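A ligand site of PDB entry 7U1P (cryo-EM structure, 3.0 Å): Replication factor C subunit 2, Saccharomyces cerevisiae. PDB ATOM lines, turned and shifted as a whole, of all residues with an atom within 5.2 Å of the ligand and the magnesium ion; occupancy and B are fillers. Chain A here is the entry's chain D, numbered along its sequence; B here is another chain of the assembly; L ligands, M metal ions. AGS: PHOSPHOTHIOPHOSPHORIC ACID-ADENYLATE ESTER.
An oxygen (O2A) of the ligand sits close to the side-chain carboxylate of Glu 159 of chain B (3.2 Å). Pro 33 touches the ligand. O of Glu 38 touches N1 of the ligand (3.9 Å). Val 39 touches the ligand. Pro 67 touches the ligand. Leu 192 touches the ligand (CD1 to N7, 3.8 Å). Leu 228 touches the ligand (CD2 to C4, 3.5 Å). Ile 232 touches the ligand. Pro 180 of chain B touches the ligand (CB to O2G, 3.6 Å). Hydrophobic or aromatic side chains within 4 Å of the ligand: Pro 33, Val 39, Pro 67, Leu 192, Leu 228, Ile 232 and Pro 180 of chain B.
Residues that only touch the magnesium ion: Arg 184 of chain B (3.6 Å).
An oxygen (O1A) of the ligand lies within hydrogen-bond range of the backbone NH (N) of Thr 72, 3.4 Å away. An oxygen (O2G) of the ligand lies within hydrogen-bond range of the guanidinium group of Arg 184 of chain B, 3.1 Å away. O3' of the ligand sits at hydrogen-bond distance from O of Val 28. An oxygen (O2A) of the ligand is in salt-bridge range of the guanidinium group (NH2) of Arg 32, 2.6 Å away. O3B of the ligand sits at hydrogen-bond distance from N of Gly 68 (2.7 Å). An oxygen (O2A) of the ligand lies within salt-bridge range of the guanidinium group (NH1) of Arg 229 (3.1 Å). NH2 of Arg 155 of chain B lies close to S1G of the ligand, at 2.9 Å. The backbone carbonyl oxygen of Thr 69 is in hydrogen-bond range of a nitrogen (N6) of the ligand, 3.2 Å away. O1A of the ligand lies within hydrogen-bond range of N of Ser 73, at 3.1 Å. The side-chain hydroxyl (OG) of Ser 73 lies within hydrogen-bond range of an oxygen (O1A) of the ligand, at 3.2 Å. ND2 of Asn 171 sits close to S1G of the ligand. The backbone NH of Lys 71 lies within hydrogen-bond range of an oxygen (O1B) of the ligand, 3.2 Å away. NZ of Lys 71 is in salt-bridge range of O1B of the ligand (3.6 Å). The backbone NH (N) of Gly 70 lies within hydrogen-bond range of an oxygen (O1B) of the ligand. The backbone NH (N) of Thr 40 lies close to a nitrogen (N1) of the ligand (3.5 Å). The backbone carbonyl oxygen (O) of Tyr 31 sits at hydrogen-bond distance from an oxygen (O2') of the ligand (3.5 Å).
The magnesium ion is bound by the side-chain hydroxyl (OG1) of Thr 72, an oxygen (O3G) of the ligand and an oxygen (O2B) of the ligand.
The backbone carbonyl oxygen of Arg 155 of chain B sits at hydrogen-bond distance from the guanidinium group of Arg 184 of chain B, at 2.7 Å. NH1 of Arg 32 is in salt-bridge range of OE2 of Glu 29 (3.0 Å). The backbone carbonyl oxygen (O) of Gly 68 lies within hydrogen-bond range of the backbone NH (N) of Leu 228 (3.4 Å). The guanidinium group (NH1) of Arg 229 is in salt-bridge range of the side-chain carboxylate (OE1) of Glu 159 of chain B, at 3.2 Å. The guanidinium group of Arg 155 of chain B is in hydrogen-bond range of the side-chain amide oxygen of Asn 171 (2.5 Å). The side-chain hydroxyl (OG1) of Thr 69 is in hydrogen-bond range of the backbone carbonyl oxygen (O) of Pro 66, 2.9 Å away. The backbone carbonyl oxygen (O) of Pro 66 sits at hydrogen-bond distance from the side-chain amino group (NZ) of Lys 71, at 2.7 Å. OE2 of Glu 159 of chain B lies within salt-bridge range of NH1 of Arg 156 of chain B (3.5 Å).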
ATOM      1  N   TRP A  27      19.141  -3.850 -19.457  1.00  0.00           N
ATOM      2  CA  TRP A  27      17.837  -3.228 -19.677  1.00  0.00           C
ATOM      3  C   TRP A  27      17.749  -2.501 -21.012  1.00  0.00           C
ATOM      4  O   TRP A  27      16.644  -2.212 -21.467  1.00  0.00           O
ATOM      5  CB  TRP A  27      17.530  -2.259 -18.525  1.00  0.00           C
ATOM      6  CG  TRP A  27      17.495  -2.914 -17.164  1.00  0.00           C
ATOM      7  CD1 TRP A  27      17.836  -4.197 -16.855  1.00  0.00           C
ATOM      8  CD2 TRP A  27      17.115  -2.296 -15.927  1.00  0.00           C
ATOM      9  NE1 TRP A  27      17.681  -4.427 -15.511  1.00  0.00           N
ATOM     10  CE2 TRP A  27      17.252  -3.271 -14.919  1.00  0.00           C
ATOM     11  CE3 TRP A  27      16.684  -1.018 -15.570  1.00  0.00           C
ATOM     12  CZ2 TRP A  27      16.963  -3.005 -13.582  1.00  0.00           C
ATOM     13  CZ3 TRP A  27      16.395  -0.752 -14.250  1.00  0.00           C
ATOM     14  CH2 TRP A  27      16.541  -1.742 -13.265  1.00  0.00           C
ATOM     15  N   VAL A  28      18.898  -2.214 -21.637  1.00  0.00           N
ATOM     16  CA  VAL A  28      18.883  -1.614 -22.964  1.00  0.00           C
ATOM     17  C   VAL A  28      18.295  -2.594 -23.981  1.00  0.00           C
ATOM     18  O   VAL A  28      17.572  -2.198 -24.904  1.00  0.00           O
ATOM     19  CB  VAL A  28      20.303  -1.176 -23.370  1.00  0.00           C
ATOM     20  CG1 VAL A  28      20.688   0.097 -22.632  1.00  0.00           C
ATOM     21  CG2 VAL A  28      21.310  -2.282 -23.097  1.00  0.00           C
ATOM     22  N   GLU A  29      18.586  -3.880 -23.808  1.00  0.00           N
ATOM     23  CA  GLU A  29      18.059  -4.921 -24.687  1.00  0.00           C
ATOM     24  C   GLU A  29      16.813  -5.605 -24.127  1.00  0.00           C
ATOM     25  O   GLU A  29      16.030  -6.160 -24.904  1.00  0.00           O
ATOM     26  CB  GLU A  29      19.126  -5.976 -24.961  1.00  0.00           C
ATOM     27  CG  GLU A  29      20.388  -5.428 -25.604  1.00  0.00           C
ATOM     28  CD  GLU A  29      20.202  -5.092 -27.062  1.00  0.00           C
ATOM     29  OE1 GLU A  29      19.380  -5.758 -27.729  1.00  0.00           O
ATOM     30  OE2 GLU A  29      20.874  -4.161 -27.549  1.00  0.00           O
ATOM     31  N   TYR A  31      14.157  -4.205 -22.670  1.00  0.00           N
ATOM     32  CA  TYR A  31      12.989  -3.433 -23.094  1.00  0.00           C
ATOM     33  C   TYR A  31      13.113  -2.915 -24.516  1.00  0.00           C
ATOM     34  O   TYR A  31      12.590  -1.842 -24.825  1.00  0.00           O
ATOM     35  CB  TYR A  31      12.735  -2.271 -22.129  1.00  0.00           C
ATOM     36  CG  TYR A  31      12.537  -2.703 -20.695  1.00  0.00           C
ATOM     37  CD1 TYR A  31      13.608  -2.792 -19.813  1.00  0.00           C
ATOM     38  CD2 TYR A  31      11.269  -3.028 -20.221  1.00  0.00           C
ATOM     39  CE1 TYR A  31      13.417  -3.185 -18.501  1.00  0.00           C
ATOM     40  CE2 TYR A  31      11.075  -3.428 -18.915  1.00  0.00           C
ATOM     41  CZ  TYR A  31      12.151  -3.510 -18.061  1.00  0.00           C
ATOM     42  OH  TYR A  31      11.937  -3.904 -16.768  1.00  0.00           O
ATOM     43  N   ARG A  32      13.786  -3.648 -25.393  1.00  0.00           N
ATOM     44  CA  ARG A  32      13.769  -3.326 -26.807  1.00  0.00           C
ATOM     45  C   ARG A  32      12.345  -3.474 -27.323  1.00  0.00           C
ATOM     46  O   ARG A  32      11.728  -4.524 -27.101  1.00  0.00           O
ATOM     47  CB  ARG A  32      14.722  -4.229 -27.589  1.00  0.00           C
ATOM     48  CG  ARG A  32      15.038  -3.761 -29.005  1.00  0.00           C
ATOM     49  CD  ARG A  32      16.302  -4.414 -29.545  1.00  0.00           C
ATOM     50  NE  ARG A  32      17.015  -3.550 -30.491  1.00  0.00           N
ATOM     51  CZ  ARG A  32      18.083  -2.831 -30.188  1.00  0.00           C
ATOM     52  NH1 ARG A  32      18.570  -2.850 -28.957  1.00  0.00           N
ATOM     53  NH2 ARG A  32      18.664  -2.079 -31.116  1.00  0.00           N
ATOM     54  N   PRO A  33      11.785  -2.466 -27.990  1.00  0.00           N
ATOM     55  CA  PRO A  33      10.372  -2.540 -28.397  1.00  0.00           C
ATOM     56  C   PRO A  33      10.053  -3.718 -29.295  1.00  0.00           C
ATOM     57  O   PRO A  33      10.542  -3.804 -30.435  1.00  0.00           O
ATOM     58  CB  PRO A  33      10.165  -1.204 -29.133  1.00  0.00           C
ATOM     59  CG  PRO A  33      11.159  -0.293 -28.503  1.00  0.00           C
ATOM     60  CD  PRO A  33      12.371  -1.155 -28.289  1.00  0.00           C
ATOM     61  N   GLU A  38       5.096   0.091 -28.832  1.00  0.00           N
ATOM     62  CA  GLU A  38       6.002   0.377 -27.736  1.00  0.00           C
ATOM     63  C   GLU A  38       6.980   1.515 -28.043  1.00  0.00           C
ATOM     64  O   GLU A  38       7.685   1.953 -27.140  1.00  0.00           O
ATOM     65  CB  GLU A  38       6.772  -0.880 -27.346  1.00  0.00           C
ATOM     66  CG  GLU A  38       5.914  -1.954 -26.698  1.00  0.00           C
ATOM     67  CD  GLU A  38       6.485  -3.349 -26.848  1.00  0.00           C
ATOM     68  OE1 GLU A  38       7.319  -3.546 -27.751  1.00  0.00           O
ATOM     69  OE2 GLU A  38       6.107  -4.233 -26.062  1.00  0.00           O
ATOM     70  N   VAL A  39       7.045   1.981 -29.294  1.00  0.00           N
ATOM     71  CA  VAL A  39       7.835   3.162 -29.601  1.00  0.00           C
ATOM     72  C   VAL A  39       7.243   4.351 -28.857  1.00  0.00           C
ATOM     73  O   VAL A  39       6.045   4.649 -28.971  1.00  0.00           O
ATOM     74  CB  VAL A  39       7.885   3.404 -31.113  1.00  0.00           C
ATOM     75  CG1 VAL A  39       8.819   4.562 -31.435  1.00  0.00           C
ATOM     76  CG2 VAL A  39       8.341   2.139 -31.828  1.00  0.00           C
ATOM     77  N   THR A  40       8.084   5.048 -28.086  1.00  0.00           N
ATOM     78  CA  THR A  40       7.586   5.994 -27.106  1.00  0.00           C
ATOM     79  C   THR A  40       7.199   7.349 -27.679  1.00  0.00           C
ATOM     80  O   THR A  40       6.163   7.898 -27.281  1.00  0.00           O
ATOM     81  CB  THR A  40       8.616   6.173 -25.977  1.00  0.00           C
ATOM     82  OG1 THR A  40       8.110   7.077 -24.991  1.00  0.00           O
ATOM     83  CG2 THR A  40       9.954   6.680 -26.516  1.00  0.00           C
ATOM     84  N   ALA A  41       7.986   7.909 -28.591  1.00  0.00           N
ATOM     85  CA  ALA A  41       7.746   9.280 -29.024  1.00  0.00           C
ATOM     86  C   ALA A  41       7.852   9.521 -30.522  1.00  0.00           C
ATOM     87  O   ALA A  41       7.452  10.604 -30.974  1.00  0.00           O
ATOM     88  CB  ALA A  41       8.710  10.236 -28.292  1.00  0.00           C
ATOM     89  N   GLN A  42       8.371   8.580 -31.298  1.00  0.00           N
ATOM     90  CA  GLN A  42       8.563   8.779 -32.732  1.00  0.00           C
ATOM     91  C   GLN A  42       7.275   8.392 -33.454  1.00  0.00           C
ATOM     92  O   GLN A  42       7.240   7.469 -34.268  1.00  0.00           O
ATOM     93  CB  GLN A  42       9.762   7.966 -33.219  1.00  0.00           C
ATOM     94  CG  GLN A  42      10.912   7.900 -32.228  1.00  0.00           C
ATOM     95  CD  GLN A  42      11.852   9.078 -32.354  1.00  0.00           C
ATOM     96  OE1 GLN A  42      11.656   9.959 -33.189  1.00  0.00           O
ATOM     97  NE2 GLN A  42      12.885   9.102 -31.516  1.00  0.00           N
ATOM     98  N   PRO A  66      19.475  11.081 -34.388  1.00  0.00           N
ATOM     99  CA  PRO A  66      20.504  10.925 -33.361  1.00  0.00           C
ATOM    100  C   PRO A  66      20.612   9.485 -32.911  1.00  0.00           C
ATOM    101  O   PRO A  66      19.634   8.720 -33.011  1.00  0.00           O
ATOM    102  CB  PRO A  66      20.010  11.839 -32.224  1.00  0.00           C
ATOM    103  CG  PRO A  66      19.089  12.809 -32.881  1.00  0.00           C
ATOM    104  CD  PRO A  66      18.425  12.040 -33.988  1.00  0.00           C
ATOM    105  N   PRO A  67      21.783   9.061 -32.419  1.00  0.00           N
ATOM    106  CA  PRO A  67      21.918   7.685 -31.929  1.00  0.00           C
ATOM    107  C   PRO A  67      21.019   7.429 -30.735  1.00  0.00           C
ATOM    108  O   PRO A  67      20.783   8.313 -29.901  1.00  0.00           O
ATOM    109  CB  PRO A  67      23.401   7.581 -31.555  1.00  0.00           C
ATOM    110  CG  PRO A  67      23.832   8.997 -31.332  1.00  0.00           C
ATOM    111  CD  PRO A  67      23.024   9.832 -32.276  1.00  0.00           C
ATOM    112  N   GLY A  68      20.518   6.198 -30.642  1.00  0.00           N
ATOM    113  CA  GLY A  68      19.672   5.813 -29.529  1.00  0.00           C
ATOM    114  C   GLY A  68      18.267   6.341 -29.550  1.00  0.00           C
ATOM    115  O   GLY A  68      17.615   6.392 -28.501  1.00  0.00           O
ATOM    116  N   THR A  69      17.754   6.744 -30.722  1.00  0.00           N
ATOM    117  CA  THR A  69      16.390   7.234 -30.827  1.00  0.00           C
ATOM    118  C   THR A  69      15.379   6.140 -31.100  1.00  0.00           C
ATOM    119  O   THR A  69      14.195   6.307 -30.754  1.00  0.00           O
ATOM    120  CB  THR A  69      16.283   8.306 -31.921  1.00  0.00           C
ATOM    121  OG1 THR A  69      16.858   7.800 -33.133  1.00  0.00           O
ATOM    122  CG2 THR A  69      17.001   9.576 -31.500  1.00  0.00           C
ATOM    123  N   GLY A  70      15.793   5.027 -31.700  1.00  0.00           N
ATOM    124  CA  GLY A  70      14.891   3.906 -31.892  1.00  0.00           C
ATOM    125  C   GLY A  70      14.690   3.479 -33.327  1.00  0.00           C
ATOM    126  O   GLY A  70      13.701   2.808 -33.639  1.00  0.00           O
ATOM    127  N   LYS A  71      15.614   3.854 -34.222  1.00  0.00           N
ATOM    128  CA  LYS A  71      15.485   3.470 -35.620  1.00  0.00           C
ATOM    129  C   LYS A  71      15.581   1.951 -35.787  1.00  0.00           C
ATOM    130  O   LYS A  71      14.738   1.335 -36.451  1.00  0.00           O
ATOM    131  CB  LYS A  71      16.559   4.163 -36.455  1.00  0.00           C
ATOM    132  CG  LYS A  71      16.721   5.647 -36.156  1.00  0.00           C
ATOM    133  CD  LYS A  71      17.765   6.282 -37.056  1.00  0.00           C
ATOM    134  CE  LYS A  71      19.105   6.407 -36.354  1.00  0.00           C
ATOM    135  NZ  LYS A  71      19.007   7.186 -35.087  1.00  0.00           N
ATOM    136  N   THR A  72      16.594   1.341 -35.185  1.00  0.00           N
ATOM    137  CA  THR A  72      16.756  -0.113 -35.287  1.00  0.00           C
ATOM    138  C   THR A  72      15.594  -0.838 -34.629  1.00  0.00           C
ATOM    139  O   THR A  72      15.081  -1.829 -35.167  1.00  0.00           O
ATOM    140  CB  THR A  72      18.080  -0.542 -34.665  1.00  0.00           C
ATOM    141  OG1 THR A  72      19.136   0.287 -35.158  1.00  0.00           O
ATOM    142  CG2 THR A  72      18.382  -1.995 -34.997  1.00  0.00           C
ATOM    143  N   SER A  73      15.156  -0.369 -33.461  1.00  0.00           N
ATOM    144  CA  SER A  73      14.018  -0.995 -32.787  1.00  0.00           C
ATOM    145  C   SER A  73      12.748  -0.875 -33.613  1.00  0.00           C
ATOM    146  O   SER A  73      11.979  -1.833 -33.732  1.00  0.00           O
ATOM    147  CB  SER A  73      13.823  -0.368 -31.407  1.00  0.00           C
ATOM    148  OG  SER A  73      14.935  -0.613 -30.564  1.00  0.00           O
ATOM    149  N   ASP A 140      21.891  -1.486 -41.812  1.00  0.00           N
ATOM    150  CA  ASP A 140      22.306  -0.699 -40.650  1.00  0.00           C
ATOM    151  C   ASP A 140      23.600   0.040 -40.948  1.00  0.00           C
ATOM    152  O   ASP A 140      24.525  -0.499 -41.561  1.00  0.00           O
ATOM    153  CB  ASP A 140      22.481  -1.614 -39.434  1.00  0.00           C
ATOM    154  CG  ASP A 140      21.261  -1.626 -38.535  1.00  0.00           C
ATOM    155  OD1 ASP A 140      20.378  -0.773 -38.714  1.00  0.00           O
ATOM    156  OD2 ASP A 140      21.197  -2.496 -37.645  1.00  0.00           O
ATOM    157  N   ILE A 169      19.433   3.016 -42.602  1.00  0.00           N
ATOM    158  CA  ILE A 169      19.560   3.653 -41.291  1.00  0.00           C
ATOM    159  C   ILE A 169      20.958   4.251 -41.192  1.00  0.00           C
ATOM    160  O   ILE A 169      21.955   3.525 -41.346  1.00  0.00           O
ATOM    161  CB  ILE A 169      19.293   2.662 -40.155  1.00  0.00           C
ATOM    162  CG1 ILE A 169      17.863   2.135 -40.234  1.00  0.00           C
ATOM    163  CG2 ILE A 169      19.542   3.327 -38.803  1.00  0.00           C
ATOM    164  CD1 ILE A 169      17.674   0.772 -39.600  1.00  0.00           C
ATOM    165  N   ASN A 171      23.233   7.577 -39.020  1.00  0.00           N
ATOM    166  CA  ASN A 171      23.219   8.674 -38.045  1.00  0.00           C
ATOM    167  C   ASN A 171      23.174  10.024 -38.750  1.00  0.00           C
ATOM    168  O   ASN A 171      22.426  10.924 -38.338  1.00  0.00           O
ATOM    169  CB  ASN A 171      24.444   8.571 -37.142  1.00  0.00           C
ATOM    170  CG  ASN A 171      24.308   7.485 -36.095  1.00  0.00           C
ATOM    171  OD1 ASN A 171      25.068   6.517 -36.071  1.00  0.00           O
ATOM    172  ND2 ASN A 171      23.323   7.634 -35.204  1.00  0.00           N
ATOM    173  N   LEU A 192      15.067  12.201 -28.146  1.00  0.00           N
ATOM    174  CA  LEU A 192      14.257  11.681 -27.045  1.00  0.00           C
ATOM    175  C   LEU A 192      14.609  12.456 -25.777  1.00  0.00           C
ATOM    176  O   LEU A 192      15.419  12.029 -24.959  1.00  0.00           O
ATOM    177  CB  LEU A 192      14.487  10.176 -26.888  1.00  0.00           C
ATOM    178  CG  LEU A 192      13.739   9.304 -27.898  1.00  0.00           C
ATOM    179  CD1 LEU A 192      13.962   7.830 -27.621  1.00  0.00           C
ATOM    180  CD2 LEU A 192      12.257   9.635 -27.885  1.00  0.00           C
ATOM    181  N   ARG A 200       7.950   6.355 -20.980  1.00  0.00           N
ATOM    182  CA  ARG A 200       8.663   5.100 -21.172  1.00  0.00           C
ATOM    183  C   ARG A 200       9.649   4.841 -20.041  1.00  0.00           C
ATOM    184  O   ARG A 200       9.743   3.720 -19.530  1.00  0.00           O
ATOM    185  CB  ARG A 200       9.389   5.113 -22.520  1.00  0.00           C
ATOM    186  CG  ARG A 200       9.883   3.747 -22.982  1.00  0.00           C
ATOM    187  CD  ARG A 200       8.857   2.652 -22.695  1.00  0.00           C
ATOM    188  NE  ARG A 200       9.329   1.337 -23.119  1.00  0.00           N
ATOM    189  CZ  ARG A 200       8.524   0.306 -23.348  1.00  0.00           C
ATOM    190  NH1 ARG A 200       7.209   0.433 -23.210  1.00  0.00           N
ATOM    191  NH2 ARG A 200       9.032  -0.860 -23.738  1.00  0.00           N
ATOM    192  N   LEU A 228      17.655   7.574 -25.315  1.00  0.00           N
ATOM    193  CA  LEU A 228      16.977   6.717 -24.350  1.00  0.00           C
ATOM    194  C   LEU A 228      17.903   5.596 -23.868  1.00  0.00           C
ATOM    195  O   LEU A 228      17.750   5.106 -22.737  1.00  0.00           O
ATOM    196  CB  LEU A 228      15.698   6.135 -24.957  1.00  0.00           C
ATOM    197  CG  LEU A 228      14.649   5.643 -23.957  1.00  0.00           C
ATOM    198  CD1 LEU A 228      14.494   6.632 -22.809  1.00  0.00           C
ATOM    199  CD2 LEU A 228      13.313   5.427 -24.652  1.00  0.00           C
ATOM    200  N   ARG A 229      18.842   5.165 -24.708  1.00  0.00           N
ATOM    201  CA  ARG A 229      19.765   4.098 -24.308  1.00  0.00           C
ATOM    202  C   ARG A 229      20.622   4.535 -23.125  1.00  0.00           C
ATOM    203  O   ARG A 229      20.795   3.770 -22.161  1.00  0.00           O
ATOM    204  CB  ARG A 229      20.654   3.710 -25.493  1.00  0.00           C
ATOM    205  CG  ARG A 229      21.219   2.293 -25.406  1.00  0.00           C
ATOM    206  CD  ARG A 229      21.683   1.791 -26.757  1.00  0.00           C
ATOM    207  NE  ARG A 229      22.157   2.871 -27.623  1.00  0.00           N
ATOM    208  CZ  ARG A 229      22.067   2.856 -28.952  1.00  0.00           C
ATOM    209  NH1 ARG A 229      21.522   1.814 -29.577  1.00  0.00           N
ATOM    210  NH2 ARG A 229      22.519   3.876 -29.662  1.00  0.00           N
ATOM    211  N   ILE A 232      18.505   4.645 -19.989  1.00  0.00           N
ATOM    212  CA  ILE A 232      18.215   3.301 -19.500  1.00  0.00           C
ATOM    213  C   ILE A 232      19.437   2.741 -18.771  1.00  0.00           C
ATOM    214  O   ILE A 232      19.311   2.151 -17.689  1.00  0.00           O
ATOM    215  CB  ILE A 232      17.782   2.401 -20.666  1.00  0.00           C
ATOM    216  CG1 ILE A 232      16.301   2.598 -20.984  1.00  0.00           C
ATOM    217  CG2 ILE A 232      18.031   0.936 -20.329  1.00  0.00           C
ATOM    218  CD1 ILE A 232      15.836   1.846 -22.207  1.00  0.00           C
ATOM    219  N   ARG B 155      29.715  -1.333 -33.624  1.00  0.00           N
ATOM    220  CA  ARG B 155      28.444  -0.747 -33.205  1.00  0.00           C
ATOM    221  C   ARG B 155      27.319  -1.767 -33.099  1.00  0.00           C
ATOM    222  O   ARG B 155      26.491  -1.669 -32.182  1.00  0.00           O
ATOM    223  CB  ARG B 155      28.045   0.359 -34.184  1.00  0.00           C
ATOM    224  CG  ARG B 155      28.214   1.770 -33.646  1.00  0.00           C
ATOM    225  CD  ARG B 155      27.764   2.798 -34.684  1.00  0.00           C
ATOM    226  NE  ARG B 155      26.313   2.785 -34.851  1.00  0.00           N
ATOM    227  CZ  ARG B 155      25.647   3.564 -35.698  1.00  0.00           C
ATOM    228  NH1 ARG B 155      26.293   4.432 -36.469  1.00  0.00           N
ATOM    229  NH2 ARG B 155      24.322   3.482 -35.776  1.00  0.00           N
ATOM    230  N   ARG B 156      27.253  -2.728 -34.018  1.00  0.00           N
ATOM    231  CA  ARG B 156      26.201  -3.744 -34.001  1.00  0.00           C
ATOM    232  C   ARG B 156      26.633  -5.027 -33.322  1.00  0.00           C
ATOM    233  O   ARG B 156      25.764  -5.809 -32.890  1.00  0.00           O
ATOM    234  CB  ARG B 156      25.739  -4.056 -35.425  1.00  0.00           C
ATOM    235  CG  ARG B 156      24.663  -3.124 -35.952  1.00  0.00           C
ATOM    236  CD  ARG B 156      23.416  -3.158 -35.077  1.00  0.00           C
ATOM    237  NE  ARG B 156      22.480  -4.185 -35.516  1.00  0.00           N
ATOM    238  CZ  ARG B 156      21.514  -4.690 -34.760  1.00  0.00           C
ATOM    239  NH1 ARG B 156      21.362  -4.272 -33.512  1.00  0.00           N
ATOM    240  NH2 ARG B 156      20.704  -5.621 -35.247  1.00  0.00           N
ATOM    241  N   GLU B 159      25.317  -5.055 -29.751  1.00  0.00           N
ATOM    242  CA  GLU B 159      23.873  -5.194 -29.545  1.00  0.00           C
ATOM    243  C   GLU B 159      23.347  -6.557 -29.976  1.00  0.00           C
ATOM    244  O   GLU B 159      22.547  -7.164 -29.272  1.00  0.00           O
ATOM    245  CB  GLU B 159      23.142  -4.080 -30.300  1.00  0.00           C
ATOM    246  CG  GLU B 159      23.170  -2.734 -29.589  1.00  0.00           C
ATOM    247  CD  GLU B 159      21.999  -1.849 -29.963  1.00  0.00           C
ATOM    248  OE1 GLU B 159      21.343  -1.320 -29.052  1.00  0.00           O
ATOM    249  OE2 GLU B 159      21.749  -1.676 -31.179  1.00  0.00           O
ATOM    250  N   PRO B 180      27.868   6.852 -30.821  1.00  0.00           N
ATOM    251  CA  PRO B 180      27.100   5.611 -30.627  1.00  0.00           C
ATOM    252  C   PRO B 180      27.783   4.600 -29.727  1.00  0.00           C
ATOM    253  O   PRO B 180      27.109   3.909 -28.950  1.00  0.00           O
ATOM    254  CB  PRO B 180      26.939   5.085 -32.052  1.00  0.00           C
ATOM    255  CG  PRO B 180      26.958   6.304 -32.895  1.00  0.00           C
ATOM    256  CD  PRO B 180      27.992   7.186 -32.256  1.00  0.00           C
ATOM    257  N   ARG B 184      26.134   3.135 -26.314  1.00  0.00           N
ATOM    258  CA  ARG B 184      25.814   1.721 -26.114  1.00  0.00           C
ATOM    259  C   ARG B 184      26.459   1.135 -24.856  1.00  0.00           C
ATOM    260  O   ARG B 184      26.123   0.008 -24.484  1.00  0.00           O
ATOM    261  CB  ARG B 184      26.260   0.911 -27.332  1.00  0.00           C
ATOM    262  CG  ARG B 184      25.170   0.657 -28.347  1.00  0.00           C
ATOM    263  CD  ARG B 184      25.699  -0.173 -29.507  1.00  0.00           C
ATOM    264  NE  ARG B 184      24.876  -0.051 -30.712  1.00  0.00           N
ATOM    265  CZ  ARG B 184      24.803   1.036 -31.470  1.00  0.00           C
ATOM    266  NH1 ARG B 184      25.522   2.111 -31.172  1.00  0.00           N
ATOM    267  NH2 ARG B 184      24.025   1.053 -32.544  1.00  0.00           N
HETATM  268  PG  AGS L   1      22.142   3.766 -33.104  1.00  0.00           P
HETATM  269  S1G AGS L   1      21.994   4.877 -34.700  1.00  0.00           S
HETATM  270  O2G AGS L   1      23.473   4.075 -32.366  1.00  0.00           O
HETATM  271  O3G AGS L   1      22.118   2.264 -33.522  1.00  0.00           O
HETATM  272  PB  AGS L   1      19.539   3.338 -32.383  1.00  0.00           P
HETATM  273  O1B AGS L   1      18.612   4.250 -33.086  1.00  0.00           O
HETATM  274  O2B AGS L   1      19.827   2.059 -33.159  1.00  0.00           O
HETATM  275  O3B AGS L   1      20.942   4.046 -32.148  1.00  0.00           O
HETATM  276  PA  AGS L   1      18.202   1.481 -30.871  1.00  0.00           P
HETATM  277  O1A AGS L   1      17.025   1.414 -31.767  1.00  0.00           O
HETATM  278  O2A AGS L   1      19.256   0.405 -31.146  1.00  0.00           O
HETATM  279  O3A AGS L   1      18.939   2.887 -30.989  1.00  0.00           O
HETATM  280  O5' AGS L   1      17.673   1.413 -29.377  1.00  0.00           O
HETATM  281  C5' AGS L   1      18.502   0.850 -28.335  1.00  0.00           C
HETATM  282  C4' AGS L   1      17.654   0.659 -27.099  1.00  0.00           C
HETATM  283  O4' AGS L   1      17.223   1.939 -26.609  1.00  0.00           O
HETATM  284  C3' AGS L   1      16.373  -0.135 -27.326  1.00  0.00           C
HETATM  285  O3' AGS L   1      16.607  -1.534 -27.165  1.00  0.00           O
HETATM  286  C2' AGS L   1      15.457   0.407 -26.227  1.00  0.00           C
HETATM  287  O2' AGS L   1      15.685  -0.217 -24.973  1.00  0.00           O
HETATM  288  C1' AGS L   1      15.878   1.883 -26.174  1.00  0.00           C
HETATM  289  N9  AGS L   1      15.086   2.755 -27.036  1.00  0.00           N
HETATM  290  C8  AGS L   1      15.548   3.577 -28.024  1.00  0.00           C
HETATM  291  N7  AGS L   1      14.614   4.264 -28.636  1.00  0.00           N
HETATM  292  C5  AGS L   1      13.448   3.864 -28.015  1.00  0.00           C
HETATM  293  C6  AGS L   1      12.103   4.225 -28.196  1.00  0.00           C
HETATM  294  N6  AGS L   1      11.678   5.099 -29.113  1.00  0.00           N
HETATM  295  N1  AGS L   1      11.175   3.636 -27.396  1.00  0.00           N
HETATM  296  C2  AGS L   1      11.588   2.755 -26.479  1.00  0.00           C
HETATM  297  N3  AGS L   1      12.829   2.340 -26.215  1.00  0.00           N
HETATM  298  C4  AGS L   1      13.721   2.937 -27.018  1.00  0.00           C
HETATM  299 MG    MG M   1      21.066   0.848 -34.641  1.00  0.00          MG
